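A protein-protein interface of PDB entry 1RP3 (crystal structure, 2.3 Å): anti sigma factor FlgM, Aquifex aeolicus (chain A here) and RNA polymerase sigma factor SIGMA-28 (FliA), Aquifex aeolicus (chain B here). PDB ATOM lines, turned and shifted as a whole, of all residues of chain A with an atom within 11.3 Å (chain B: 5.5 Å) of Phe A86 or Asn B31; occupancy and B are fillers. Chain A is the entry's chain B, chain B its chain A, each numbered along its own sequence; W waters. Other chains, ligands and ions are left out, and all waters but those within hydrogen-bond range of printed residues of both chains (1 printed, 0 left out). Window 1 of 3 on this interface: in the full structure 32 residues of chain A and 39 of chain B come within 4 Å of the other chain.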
ATOM      1  N   SER A  47     -21.525 -17.623  -4.749  1.00  0.00           N
ATOM      2  CA  SER A  47     -21.571 -16.390  -3.980  1.00  0.00           C
ATOM      3  C   SER A  47     -22.672 -15.451  -4.446  1.00  0.00           C
ATOM      4  O   SER A  47     -22.565 -14.233  -4.303  1.00  0.00           O
ATOM      5  CB  SER A  47     -20.204 -15.694  -4.013  1.00  0.00           C
ATOM      6  OG  SER A  47     -19.735 -15.515  -5.335  1.00  0.00           O
ATOM      7  N   ASP A  50     -24.842 -13.653  -1.272  1.00  0.00           N
ATOM      8  CA  ASP A  50     -23.905 -13.265  -0.220  1.00  0.00           C
ATOM      9  C   ASP A  50     -24.243 -12.016   0.595  1.00  0.00           C
ATOM     10  O   ASP A  50     -24.286 -10.896   0.077  1.00  0.00           O
ATOM     11  CB  ASP A  50     -22.483 -13.150  -0.782  1.00  0.00           C
ATOM     12  CG  ASP A  50     -21.776 -14.489  -0.867  1.00  0.00           C
ATOM     13  OD1 ASP A  50     -22.450 -15.541  -0.767  1.00  0.00           O
ATOM     14  OD2 ASP A  50     -20.539 -14.483  -1.027  1.00  0.00           O
ATOM     15  N   GLU A  52     -22.621 -11.847   3.743  1.00  0.00           N
ATOM     16  CA  GLU A  52     -21.564 -12.243   4.681  1.00  0.00           C
ATOM     17  C   GLU A  52     -21.743 -11.990   6.183  1.00  0.00           C
ATOM     18  O   GLU A  52     -21.713 -12.933   6.980  1.00  0.00           O
ATOM     19  CB  GLU A  52     -20.219 -11.683   4.211  1.00  0.00           C
ATOM     20  N   LEU A  56     -21.767 -10.187  12.752  1.00  0.00           N
ATOM     21  CA  LEU A  56     -20.501  -9.468  12.781  1.00  0.00           C
ATOM     22  C   LEU A  56     -20.544  -8.261  13.721  1.00  0.00           C
ATOM     23  O   LEU A  56     -19.720  -8.159  14.633  1.00  0.00           O
ATOM     24  CB  LEU A  56     -20.121  -9.054  11.351  1.00  0.00           C
ATOM     25  CG  LEU A  56     -18.729  -8.523  10.978  1.00  0.00           C
ATOM     26  CD1 LEU A  56     -18.763  -7.011  10.795  1.00  0.00           C
ATOM     27  CD2 LEU A  56     -17.686  -8.954  11.998  1.00  0.00           C
ATOM     28  N   LYS A  59     -21.052  -9.462  17.355  1.00  0.00           N
ATOM     29  CA  LYS A  59     -19.853 -10.166  17.802  1.00  0.00           C
ATOM     30  C   LYS A  59     -18.782  -9.169  18.221  1.00  0.00           C
ATOM     31  O   LYS A  59     -18.093  -9.371  19.222  1.00  0.00           O
ATOM     32  CB  LYS A  59     -19.315 -11.055  16.679  1.00  0.00           C
ATOM     33  CG  LYS A  59     -18.114 -11.898  17.068  1.00  0.00           C
ATOM     34  CD  LYS A  59     -17.705 -12.815  15.935  1.00  0.00           C
ATOM     35  CE  LYS A  59     -16.615 -13.776  16.373  1.00  0.00           C
ATOM     36  NZ  LYS A  59     -16.319 -14.777  15.314  1.00  0.00           N
ATOM     37  N   GLU A  77      -3.659 -21.832  23.713  1.00  0.00           N
ATOM     38  CA  GLU A  77      -4.439 -22.889  23.075  1.00  0.00           C
ATOM     39  C   GLU A  77      -5.287 -22.311  21.942  1.00  0.00           C
ATOM     40  O   GLU A  77      -5.212 -22.769  20.802  1.00  0.00           O
ATOM     41  CB  GLU A  77      -5.328 -23.597  24.104  1.00  0.00           C
ATOM     42  N   LYS A  78      -6.066 -21.280  22.255  1.00  0.00           N
ATOM     43  CA  LYS A  78      -6.927 -20.626  21.275  1.00  0.00           C
ATOM     44  C   LYS A  78      -6.156 -20.071  20.072  1.00  0.00           C
ATOM     45  O   LYS A  78      -6.589 -20.215  18.934  1.00  0.00           O
ATOM     46  CB  LYS A  78      -7.729 -19.515  21.950  1.00  0.00           C
ATOM     47  CG  LYS A  78      -8.751 -20.025  22.951  1.00  0.00           C
ATOM     48  CD  LYS A  78      -9.495 -18.888  23.636  1.00  0.00           C
ATOM     49  CE  LYS A  78     -10.524 -19.432  24.621  1.00  0.00           C
ATOM     50  NZ  LYS A  78     -11.265 -18.346  25.325  1.00  0.00           N
ATOM     51  N   VAL A  79      -5.017 -19.436  20.333  1.00  0.00           N
ATOM     52  CA  VAL A  79      -4.186 -18.866  19.275  1.00  0.00           C
ATOM     53  C   VAL A  79      -3.662 -19.992  18.396  1.00  0.00           C
ATOM     54  O   VAL A  79      -3.541 -19.842  17.181  1.00  0.00           O
ATOM     55  CB  VAL A  79      -2.991 -18.073  19.865  1.00  0.00           C
ATOM     56  CG1 VAL A  79      -2.118 -17.505  18.759  1.00  0.00           C
ATOM     57  CG2 VAL A  79      -3.496 -16.954  20.762  1.00  0.00           C
ATOM     58  N   VAL A  80      -3.331 -21.115  19.027  1.00  0.00           N
ATOM     59  CA  VAL A  80      -2.832 -22.283  18.311  1.00  0.00           C
ATOM     60  C   VAL A  80      -3.956 -22.854  17.455  1.00  0.00           C
ATOM     61  O   VAL A  80      -3.752 -23.155  16.278  1.00  0.00           O
ATOM     62  CB  VAL A  80      -2.291 -23.355  19.295  1.00  0.00           C
ATOM     63  CG1 VAL A  80      -2.222 -24.734  18.637  1.00  0.00           C
ATOM     64  CG2 VAL A  80      -0.916 -22.942  19.777  1.00  0.00           C
ATOM     65  N   LYS A  81      -5.143 -22.983  18.042  1.00  0.00           N
ATOM     66  CA  LYS A  81      -6.299 -23.501  17.314  1.00  0.00           C
ATOM     67  C   LYS A  81      -6.583 -22.587  16.122  1.00  0.00           C
ATOM     68  O   LYS A  81      -6.845 -23.064  15.013  1.00  0.00           O
ATOM     69  CB  LYS A  81      -7.523 -23.587  18.231  1.00  0.00           C
ATOM     70  N   GLY A  82      -6.448 -21.282  16.350  1.00  0.00           N
ATOM     71  CA  GLY A  82      -6.680 -20.300  15.305  1.00  0.00           C
ATOM     72  C   GLY A  82      -5.754 -20.435  14.109  1.00  0.00           C
ATOM     73  O   GLY A  82      -6.197 -20.573  12.962  1.00  0.00           O
ATOM     74  N   LEU A  83      -4.458 -20.418  14.382  1.00  0.00           N
ATOM     75  CA  LEU A  83      -3.453 -20.523  13.336  1.00  0.00           C
ATOM     76  C   LEU A  83      -3.500 -21.853  12.602  1.00  0.00           C
ATOM     77  O   LEU A  83      -3.465 -21.893  11.370  1.00  0.00           O
ATOM     78  CB  LEU A  83      -2.058 -20.274  13.913  1.00  0.00           C
ATOM     79  CG  LEU A  83      -1.886 -18.921  14.605  1.00  0.00           C
ATOM     80  CD1 LEU A  83      -0.641 -18.931  15.484  1.00  0.00           C
ATOM     81  CD2 LEU A  83      -1.825 -17.807  13.563  1.00  0.00           C
ATOM     82  N   ILE A  84      -3.615 -22.940  13.352  1.00  0.00           N
ATOM     83  CA  ILE A  84      -3.647 -24.253  12.733  1.00  0.00           C
ATOM     84  C   ILE A  84      -4.874 -24.444  11.849  1.00  0.00           C
ATOM     85  O   ILE A  84      -4.757 -24.949  10.740  1.00  0.00           O
ATOM     86  CB  ILE A  84      -3.530 -25.384  13.783  1.00  0.00           C
ATOM     87  CG1 ILE A  84      -2.133 -25.347  14.399  1.00  0.00           C
ATOM     88  CG2 ILE A  84      -3.781 -26.762  13.132  1.00  0.00           C
ATOM     89  CD1 ILE A  84      -1.894 -26.398  15.447  1.00  0.00           C
ATOM     90  N   GLU A  85      -6.042 -24.040  12.335  1.00  0.00           N
ATOM     91  CA  GLU A  85      -7.280 -24.160  11.564  1.00  0.00           C
ATOM     92  C   GLU A  85      -7.215 -23.314  10.294  1.00  0.00           C
ATOM     93  O   GLU A  85      -7.718 -23.714   9.250  1.00  0.00           O
ATOM     94  CB  GLU A  85      -8.479 -23.721  12.413  1.00  0.00           C
ATOM     95  CG  GLU A  85      -9.695 -24.634  12.306  1.00  0.00           C
ATOM     96  CD  GLU A  85     -10.443 -24.762  13.631  1.00  0.00           C
ATOM     97  OE1 GLU A  85     -10.713 -23.717  14.273  1.00  0.00           O
ATOM     98  OE2 GLU A  85     -10.754 -25.911  14.030  1.00  0.00           O
ATOM     99  N   PHE A  86      -6.583 -22.147  10.381  1.00  0.00           N
ATOM    100  CA  PHE A  86      -6.467 -21.270   9.233  1.00  0.00           C
ATOM    101  C   PHE A  86      -5.495 -21.781   8.174  1.00  0.00           C
ATOM    102  O   PHE A  86      -5.805 -21.762   6.978  1.00  0.00           O
ATOM    103  CB  PHE A  86      -6.047 -19.863   9.669  1.00  0.00           C
ATOM    104  CG  PHE A  86      -5.859 -18.911   8.524  1.00  0.00           C
ATOM    105  CD1 PHE A  86      -6.958 -18.297   7.920  1.00  0.00           C
ATOM    106  CD2 PHE A  86      -4.588 -18.641   8.031  1.00  0.00           C
ATOM    107  CE1 PHE A  86      -6.791 -17.433   6.831  1.00  0.00           C
ATOM    108  CE2 PHE A  86      -4.411 -17.774   6.937  1.00  0.00           C
ATOM    109  CZ  PHE A  86      -5.517 -17.170   6.341  1.00  0.00           C
ATOM    110  N   PHE A  87      -4.319 -22.226   8.607  1.00  0.00           N
ATOM    111  CA  PHE A  87      -3.306 -22.692   7.659  1.00  0.00           C
ATOM    112  C   PHE A  87      -3.419 -24.124   7.112  1.00  0.00           C
ATOM    113  O   PHE A  87      -3.170 -24.351   5.925  1.00  0.00           O
ATOM    114  CB  PHE A  87      -1.904 -22.425   8.207  1.00  0.00           C
ATOM    115  CG  PHE A  87      -1.553 -20.964   8.289  1.00  0.00           C
ATOM    116  CD1 PHE A  87      -1.141 -20.276   7.154  1.00  0.00           C
ATOM    117  CD2 PHE A  87      -1.603 -20.284   9.501  1.00  0.00           C
ATOM    118  CE1 PHE A  87      -0.780 -18.935   7.217  1.00  0.00           C
ATOM    119  CE2 PHE A  87      -1.240 -18.930   9.577  1.00  0.00           C
ATOM    120  CZ  PHE A  87      -0.827 -18.260   8.428  1.00  0.00           C
ATOM    121  N   THR A  88      -3.837 -25.070   7.952  1.00  0.00           N
ATOM    122  CA  THR A  88      -3.960 -26.473   7.539  1.00  0.00           C
ATOM    123  C   THR A  88      -5.358 -26.894   7.067  1.00  0.00           C
ATOM    124  O   THR A  88      -5.447 -27.908   6.341  1.00  0.00           O
ATOM    125  CB  THR A  88      -3.531 -27.431   8.677  1.00  0.00           C
ATOM    126  OG1 THR A  88      -4.527 -27.433   9.715  1.00  0.00           O
ATOM    127  CG2 THR A  88      -2.176 -27.013   9.241  1.00  0.00           C
ATOM    128  OXT THR A  88      -6.351 -26.252   7.469  1.00  0.00           O
ATOM    129  N   LYS B  26     -15.865 -22.256  -1.146  1.00  0.00           N
ATOM    130  CA  LYS B  26     -16.433 -20.937  -0.898  1.00  0.00           C
ATOM    131  C   LYS B  26     -15.982 -20.485   0.481  1.00  0.00           C
ATOM    132  O   LYS B  26     -15.436 -19.394   0.639  1.00  0.00           O
ATOM    133  CB  LYS B  26     -17.964 -21.020  -0.929  1.00  0.00           C
ATOM    134  CG  LYS B  26     -18.722 -19.757  -1.316  1.00  0.00           C
ATOM    135  CD  LYS B  26     -18.202 -18.512  -0.661  1.00  0.00           C
ATOM    136  CE  LYS B  26     -19.294 -17.470  -0.472  1.00  0.00           C
ATOM    137  NZ  LYS B  26     -20.263 -17.837   0.619  1.00  0.00           N
ATOM    138  N   ALA B  27     -16.186 -21.349   1.470  1.00  0.00           N
ATOM    139  CA  ALA B  27     -15.828 -21.050   2.847  1.00  0.00           C
ATOM    140  C   ALA B  27     -14.356 -20.671   3.019  1.00  0.00           C
ATOM    141  O   ALA B  27     -14.025 -19.683   3.680  1.00  0.00           O
ATOM    142  CB  ALA B  27     -16.180 -22.211   3.709  1.00  0.00           C
ATOM    143  N   ILE B  28     -13.488 -21.410   2.333  1.00  0.00           N
ATOM    144  CA  ILE B  28     -12.051 -21.188   2.394  1.00  0.00           C
ATOM    145  C   ILE B  28     -11.662 -19.880   1.711  1.00  0.00           C
ATOM    146  O   ILE B  28     -10.858 -19.120   2.242  1.00  0.00           O
ATOM    147  CB  ILE B  28     -11.279 -22.408   1.795  1.00  0.00           C
ATOM    148  CG1 ILE B  28     -11.478 -23.615   2.717  1.00  0.00           C
ATOM    149  CG2 ILE B  28      -9.792 -22.099   1.661  1.00  0.00           C
ATOM    150  CD1 ILE B  28     -11.062 -24.960   2.118  1.00  0.00           C
ATOM    151  N   ALA B  29     -12.261 -19.599   0.560  1.00  0.00           N
ATOM    152  CA  ALA B  29     -11.963 -18.378  -0.178  1.00  0.00           C
ATOM    153  C   ALA B  29     -12.417 -17.157   0.608  1.00  0.00           C
ATOM    154  O   ALA B  29     -11.699 -16.159   0.710  1.00  0.00           O
ATOM    155  CB  ALA B  29     -12.634 -18.423  -1.550  1.00  0.00           C
ATOM    156  N   THR B  30     -13.584 -17.270   1.232  1.00  0.00           N
ATOM    157  CA  THR B  30     -14.131 -16.179   2.028  1.00  0.00           C
ATOM    158  C   THR B  30     -13.209 -15.899   3.231  1.00  0.00           C
ATOM    159  O   THR B  30     -12.912 -14.749   3.546  1.00  0.00           O
ATOM    160  CB  THR B  30     -15.571 -16.534   2.533  1.00  0.00           C
ATOM    161  OG1 THR B  30     -16.422 -16.791   1.412  1.00  0.00           O
ATOM    162  CG2 THR B  30     -16.181 -15.395   3.340  1.00  0.00           C
ATOM    163  N   ASN B  31     -12.759 -16.956   3.896  1.00  0.00           N
ATOM    164  CA  ASN B  31     -11.898 -16.812   5.059  1.00  0.00           C
ATOM    165  C   ASN B  31     -10.547 -16.199   4.718  1.00  0.00           C
ATOM    166  O   ASN B  31     -10.014 -15.381   5.480  1.00  0.00           O
ATOM    167  CB  ASN B  31     -11.723 -18.145   5.769  1.00  0.00           C
ATOM    168  CG  ASN B  31     -11.035 -17.996   7.096  1.00  0.00           C
ATOM    169  OD1 ASN B  31      -9.953 -18.537   7.299  1.00  0.00           O
ATOM    170  ND2 ASN B  31     -11.641 -17.233   8.006  1.00  0.00           N
ATOM    171  N   ILE B  32     -10.011 -16.573   3.559  1.00  0.00           N
ATOM    172  CA  ILE B  32      -8.739 -16.033   3.109  1.00  0.00           C
ATOM    173  C   ILE B  32      -8.960 -14.581   2.686  1.00  0.00           C
ATOM    174  O   ILE B  32      -8.120 -13.726   2.948  1.00  0.00           O
ATOM    175  CB  ILE B  32      -8.143 -16.887   1.958  1.00  0.00           C
ATOM    176  CG1 ILE B  32      -7.709 -18.246   2.501  1.00  0.00           C
ATOM    177  CG2 ILE B  32      -6.956 -16.214   1.318  1.00  0.00           C
ATOM    178  CD1 ILE B  32      -7.298 -19.229   1.422  1.00  0.00           C
ATOM    179  N   LYS B  33     -10.128 -14.298   2.107  1.00  0.00           N
ATOM    180  CA  LYS B  33     -10.464 -12.940   1.669  1.00  0.00           C
ATOM    181  C   LYS B  33     -10.406 -11.916   2.800  1.00  0.00           C
ATOM    182  O   LYS B  33     -10.176 -10.733   2.564  1.00  0.00           O
ATOM    183  CB  LYS B  33     -11.846 -12.901   1.010  1.00  0.00           C
ATOM    184  CG  LYS B  33     -11.818 -13.043  -0.500  1.00  0.00           C
ATOM    185  CD  LYS B  33     -11.296 -11.788  -1.175  1.00  0.00           C
ATOM    186  CE  LYS B  33     -12.268 -10.625  -1.033  1.00  0.00           C
ATOM    187  NZ  LYS B  33     -11.718  -9.344  -1.589  1.00  0.00           N
ATOM    188  N   LYS B  34     -10.597 -12.364   4.032  1.00  0.00           N
ATOM    189  CA  LYS B  34     -10.553 -11.446   5.170  1.00  0.00           C
ATOM    190  C   LYS B  34      -9.163 -10.846   5.407  1.00  0.00           C
ATOM    191  O   LYS B  34      -9.023  -9.840   6.106  1.00  0.00           O
ATOM    192  CB  LYS B  34     -11.020 -12.143   6.441  1.00  0.00           C
ATOM    193  CG  LYS B  34     -12.478 -12.550   6.445  1.00  0.00           C
ATOM    194  CD  LYS B  34     -12.784 -13.335   7.718  1.00  0.00           C
ATOM    195  CE  LYS B  34     -14.269 -13.599   7.879  1.00  0.00           C
ATOM    196  NZ  LYS B  34     -14.543 -14.279   9.168  1.00  0.00           N
ATOM    197  N   HIS B  35      -8.146 -11.450   4.799  1.00  0.00           N
ATOM    198  CA  HIS B  35      -6.770 -10.997   4.959  1.00  0.00           C
ATOM    199  C   HIS B  35      -6.196 -10.414   3.676  1.00  0.00           C
ATOM    200  O   HIS B  35      -5.009 -10.112   3.603  1.00  0.00           O
ATOM    201  CB  HIS B  35      -5.887 -12.172   5.366  1.00  0.00           C
ATOM    202  CG  HIS B  35      -6.399 -12.929   6.555  1.00  0.00           C
ATOM    203  ND1 HIS B  35      -5.816 -12.821   7.796  1.00  0.00           N
ATOM    204  CD2 HIS B  35      -7.409 -13.808   6.675  1.00  0.00           C
ATOM    205  CE1 HIS B  35      -6.456 -13.615   8.640  1.00  0.00           C
ATOM    206  NE2 HIS B  35      -7.425 -14.223   7.995  1.00  0.00           N
ATOM    207  N   LYS B  77      -6.663 -25.027  -0.244  1.00  0.00           N
ATOM    208  CA  LYS B  77      -5.864 -23.929   0.320  1.00  0.00           C
ATOM    209  C   LYS B  77      -4.556 -23.806  -0.458  1.00  0.00           C
ATOM    210  O   LYS B  77      -4.158 -22.710  -0.851  1.00  0.00           O
ATOM    211  CB  LYS B  77      -5.573 -24.167   1.810  1.00  0.00           C
ATOM    212  CG  LYS B  77      -6.823 -24.133   2.688  1.00  0.00           C
ATOM    213  CD  LYS B  77      -6.521 -24.161   4.181  1.00  0.00           C
ATOM    214  CE  LYS B  77      -7.808 -23.984   5.001  1.00  0.00           C
ATOM    215  NZ  LYS B  77      -7.570 -23.769   6.464  1.00  0.00           N
ATOM    216  N   TYR B  81      -3.236 -20.507  -2.395  1.00  0.00           N
ATOM    217  CA  TYR B  81      -1.979 -19.862  -2.010  1.00  0.00           C
ATOM    218  C   TYR B  81      -0.969 -19.946  -3.154  1.00  0.00           C
ATOM    219  O   TYR B  81      -0.135 -19.048  -3.319  1.00  0.00           O
ATOM    220  CB  TYR B  81      -1.420 -20.462  -0.715  1.00  0.00           C
ATOM    221  CG  TYR B  81      -2.147 -19.975   0.519  1.00  0.00           C
ATOM    222  CD1 TYR B  81      -2.002 -18.660   0.959  1.00  0.00           C
ATOM    223  CD2 TYR B  81      -3.008 -20.808   1.216  1.00  0.00           C
ATOM    224  CE1 TYR B  81      -2.699 -18.188   2.062  1.00  0.00           C
ATOM    225  CE2 TYR B  81      -3.710 -20.351   2.314  1.00  0.00           C
ATOM    226  CZ  TYR B  81      -3.548 -19.038   2.734  1.00  0.00           C
ATOM    227  OH  TYR B  81      -4.217 -18.587   3.844  1.00  0.00           O
ATOM    228  N   ILE B 144       1.635 -13.500   5.711  1.00  0.00           N
ATOM    229  CA  ILE B 144       0.762 -14.662   5.770  1.00  0.00           C
ATOM    230  C   ILE B 144       1.333 -15.706   4.826  1.00  0.00           C
ATOM    231  O   ILE B 144       1.425 -16.877   5.174  1.00  0.00           O
ATOM    232  CB  ILE B 144      -0.687 -14.296   5.385  1.00  0.00           C
ATOM    233  CG1 ILE B 144      -1.364 -13.663   6.592  1.00  0.00           C
ATOM    234  CG2 ILE B 144      -1.477 -15.529   4.915  1.00  0.00           C
ATOM    235  CD1 ILE B 144      -2.659 -12.992   6.272  1.00  0.00           C
ATOM    236  N   PHE B 200      -7.411 -14.591  14.083  1.00  0.00           N
ATOM    237  CA  PHE B 200      -7.496 -15.977  13.646  1.00  0.00           C
ATOM    238  C   PHE B 200      -8.421 -16.892  14.416  1.00  0.00           C
ATOM    239  O   PHE B 200      -9.000 -17.805  13.834  1.00  0.00           O
ATOM    240  CB  PHE B 200      -6.100 -16.600  13.595  1.00  0.00           C
ATOM    241  CG  PHE B 200      -5.188 -15.959  12.593  1.00  0.00           C
ATOM    242  CD1 PHE B 200      -4.393 -14.887  12.954  1.00  0.00           C
ATOM    243  CD2 PHE B 200      -5.081 -16.467  11.302  1.00  0.00           C
ATOM    244  CE1 PHE B 200      -3.499 -14.322  12.045  1.00  0.00           C
ATOM    245  CE2 PHE B 200      -4.188 -15.908  10.381  1.00  0.00           C
ATOM    246  CZ  PHE B 200      -3.393 -14.835  10.758  1.00  0.00           C
ATOM    247  N   GLU B 203     -11.695 -14.943  14.029  1.00  0.00           N
ATOM    248  CA  GLU B 203     -11.906 -14.756  12.594  1.00  0.00           C
ATOM    249  C   GLU B 203     -12.463 -13.377  12.243  1.00  0.00           C
ATOM    250  O   GLU B 203     -13.468 -13.236  11.546  1.00  0.00           O
ATOM    251  CB  GLU B 203     -12.783 -15.875  12.032  1.00  0.00           C
ATOM    252  CG  GLU B 203     -12.167 -17.261  12.197  1.00  0.00           C
ATOM    253  CD  GLU B 203     -13.013 -18.367  11.593  1.00  0.00           C
ATOM    254  OE1 GLU B 203     -14.206 -18.489  11.949  1.00  0.00           O
ATOM    255  OE2 GLU B 203     -12.479 -19.123  10.758  1.00  0.00           O
HETATM  256  O   HOH W   1      -5.667 -20.366   4.769  1.00  0.00           O
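The side-chain hydroxyl (OG1) of Thr A88 lies within hydrogen-bond range of the backbone carbonyl oxygen (O) of Ile A84, 2.7 Å away.
O of Lys B26 lies within hydrogen-bond range of OG1 of Thr B30, at 2.9 Å.
OE2 of Glu B203 is in hydrogen-bond range of ND2 of Asn B31 (3.4 Å).
Along chain B the printed residues that touch a printed residue of chain A span positions 26 to 200.
Along chain A the printed residues that touch a printed residue of chain B span positions 50 to 88.
Among the printed residues, Asp or Glu carboxylates within 4 Å of a Lys or Arg side-chain nitrogen of the other chain: Asp A50 with Lys B26 (3.5 Å).
The side-chain amino group (NZ) of Lys B77 is in salt-bridge range of the chain-end carboxylate (OXT) of Thr A88.
The side-chain amino group of Lys B77 is in hydrogen-bond range of the backbone carbonyl oxygen of Phe A86 (2.7 Å).
The side-chain amino group (NZ) of Lys B77 sits at hydrogen-bond distance from the backbone carbonyl oxygen (O) of Glu A85, 2.8 Å away.
The side-chain carboxylate (OD1) of Asp A50 is in salt-bridge range of the side-chain amino group (NZ) of Lys B26 (3.5 Å).
Gly A82 touches Phe B200.
CD1 of Phe B200 touches CD2 of Leu A83 (3.9 Å).
Asn B31 touches Phe A86 (OD1 to CD1, 3.1 Å).
CE1 of Phe A86 touches NE2 of His B35, at 3.5 Å.
OH of Tyr B81 touches CZ of Phe A86 (3.2 Å).
CE2 of Phe B200 touches CD2 of Phe A86 (3.6 Å).
Lys B77 touches Phe A87.
CE1 of Phe A87 touches O of Ile B144 (3.6 Å).
Water W1 bridges OH of Tyr B81 (2.5 Å) and O of Phe A86 (2.6 Å).
Lys A59 touches none of the printed residues of chain B.
Of the printed residues of chain B, Leu A83 touches Phe B200.
Of the printed residues of chain A, Lys B26 touches Asp A50.
No residue of chain A comes within 4 Å of Ile B32.
No residue of chain A comes within 4 Å of Lys B34.
Phe B200 touches just these residues of chain A: Gly A82 (3.7 Å), Leu A83 (3.9 Å) and Phe A86 (3.6 Å).
The nearest residue of chain B that does not touch Phe A86 is Ile B144 (4.2 Å).
The nearest residue of chain A that does not touch Asn B31 is Glu A85 (6.0 Å).
The nearest printed residue of chain B that does not touch Glu A85 is Asn B31 (6.0 Å).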
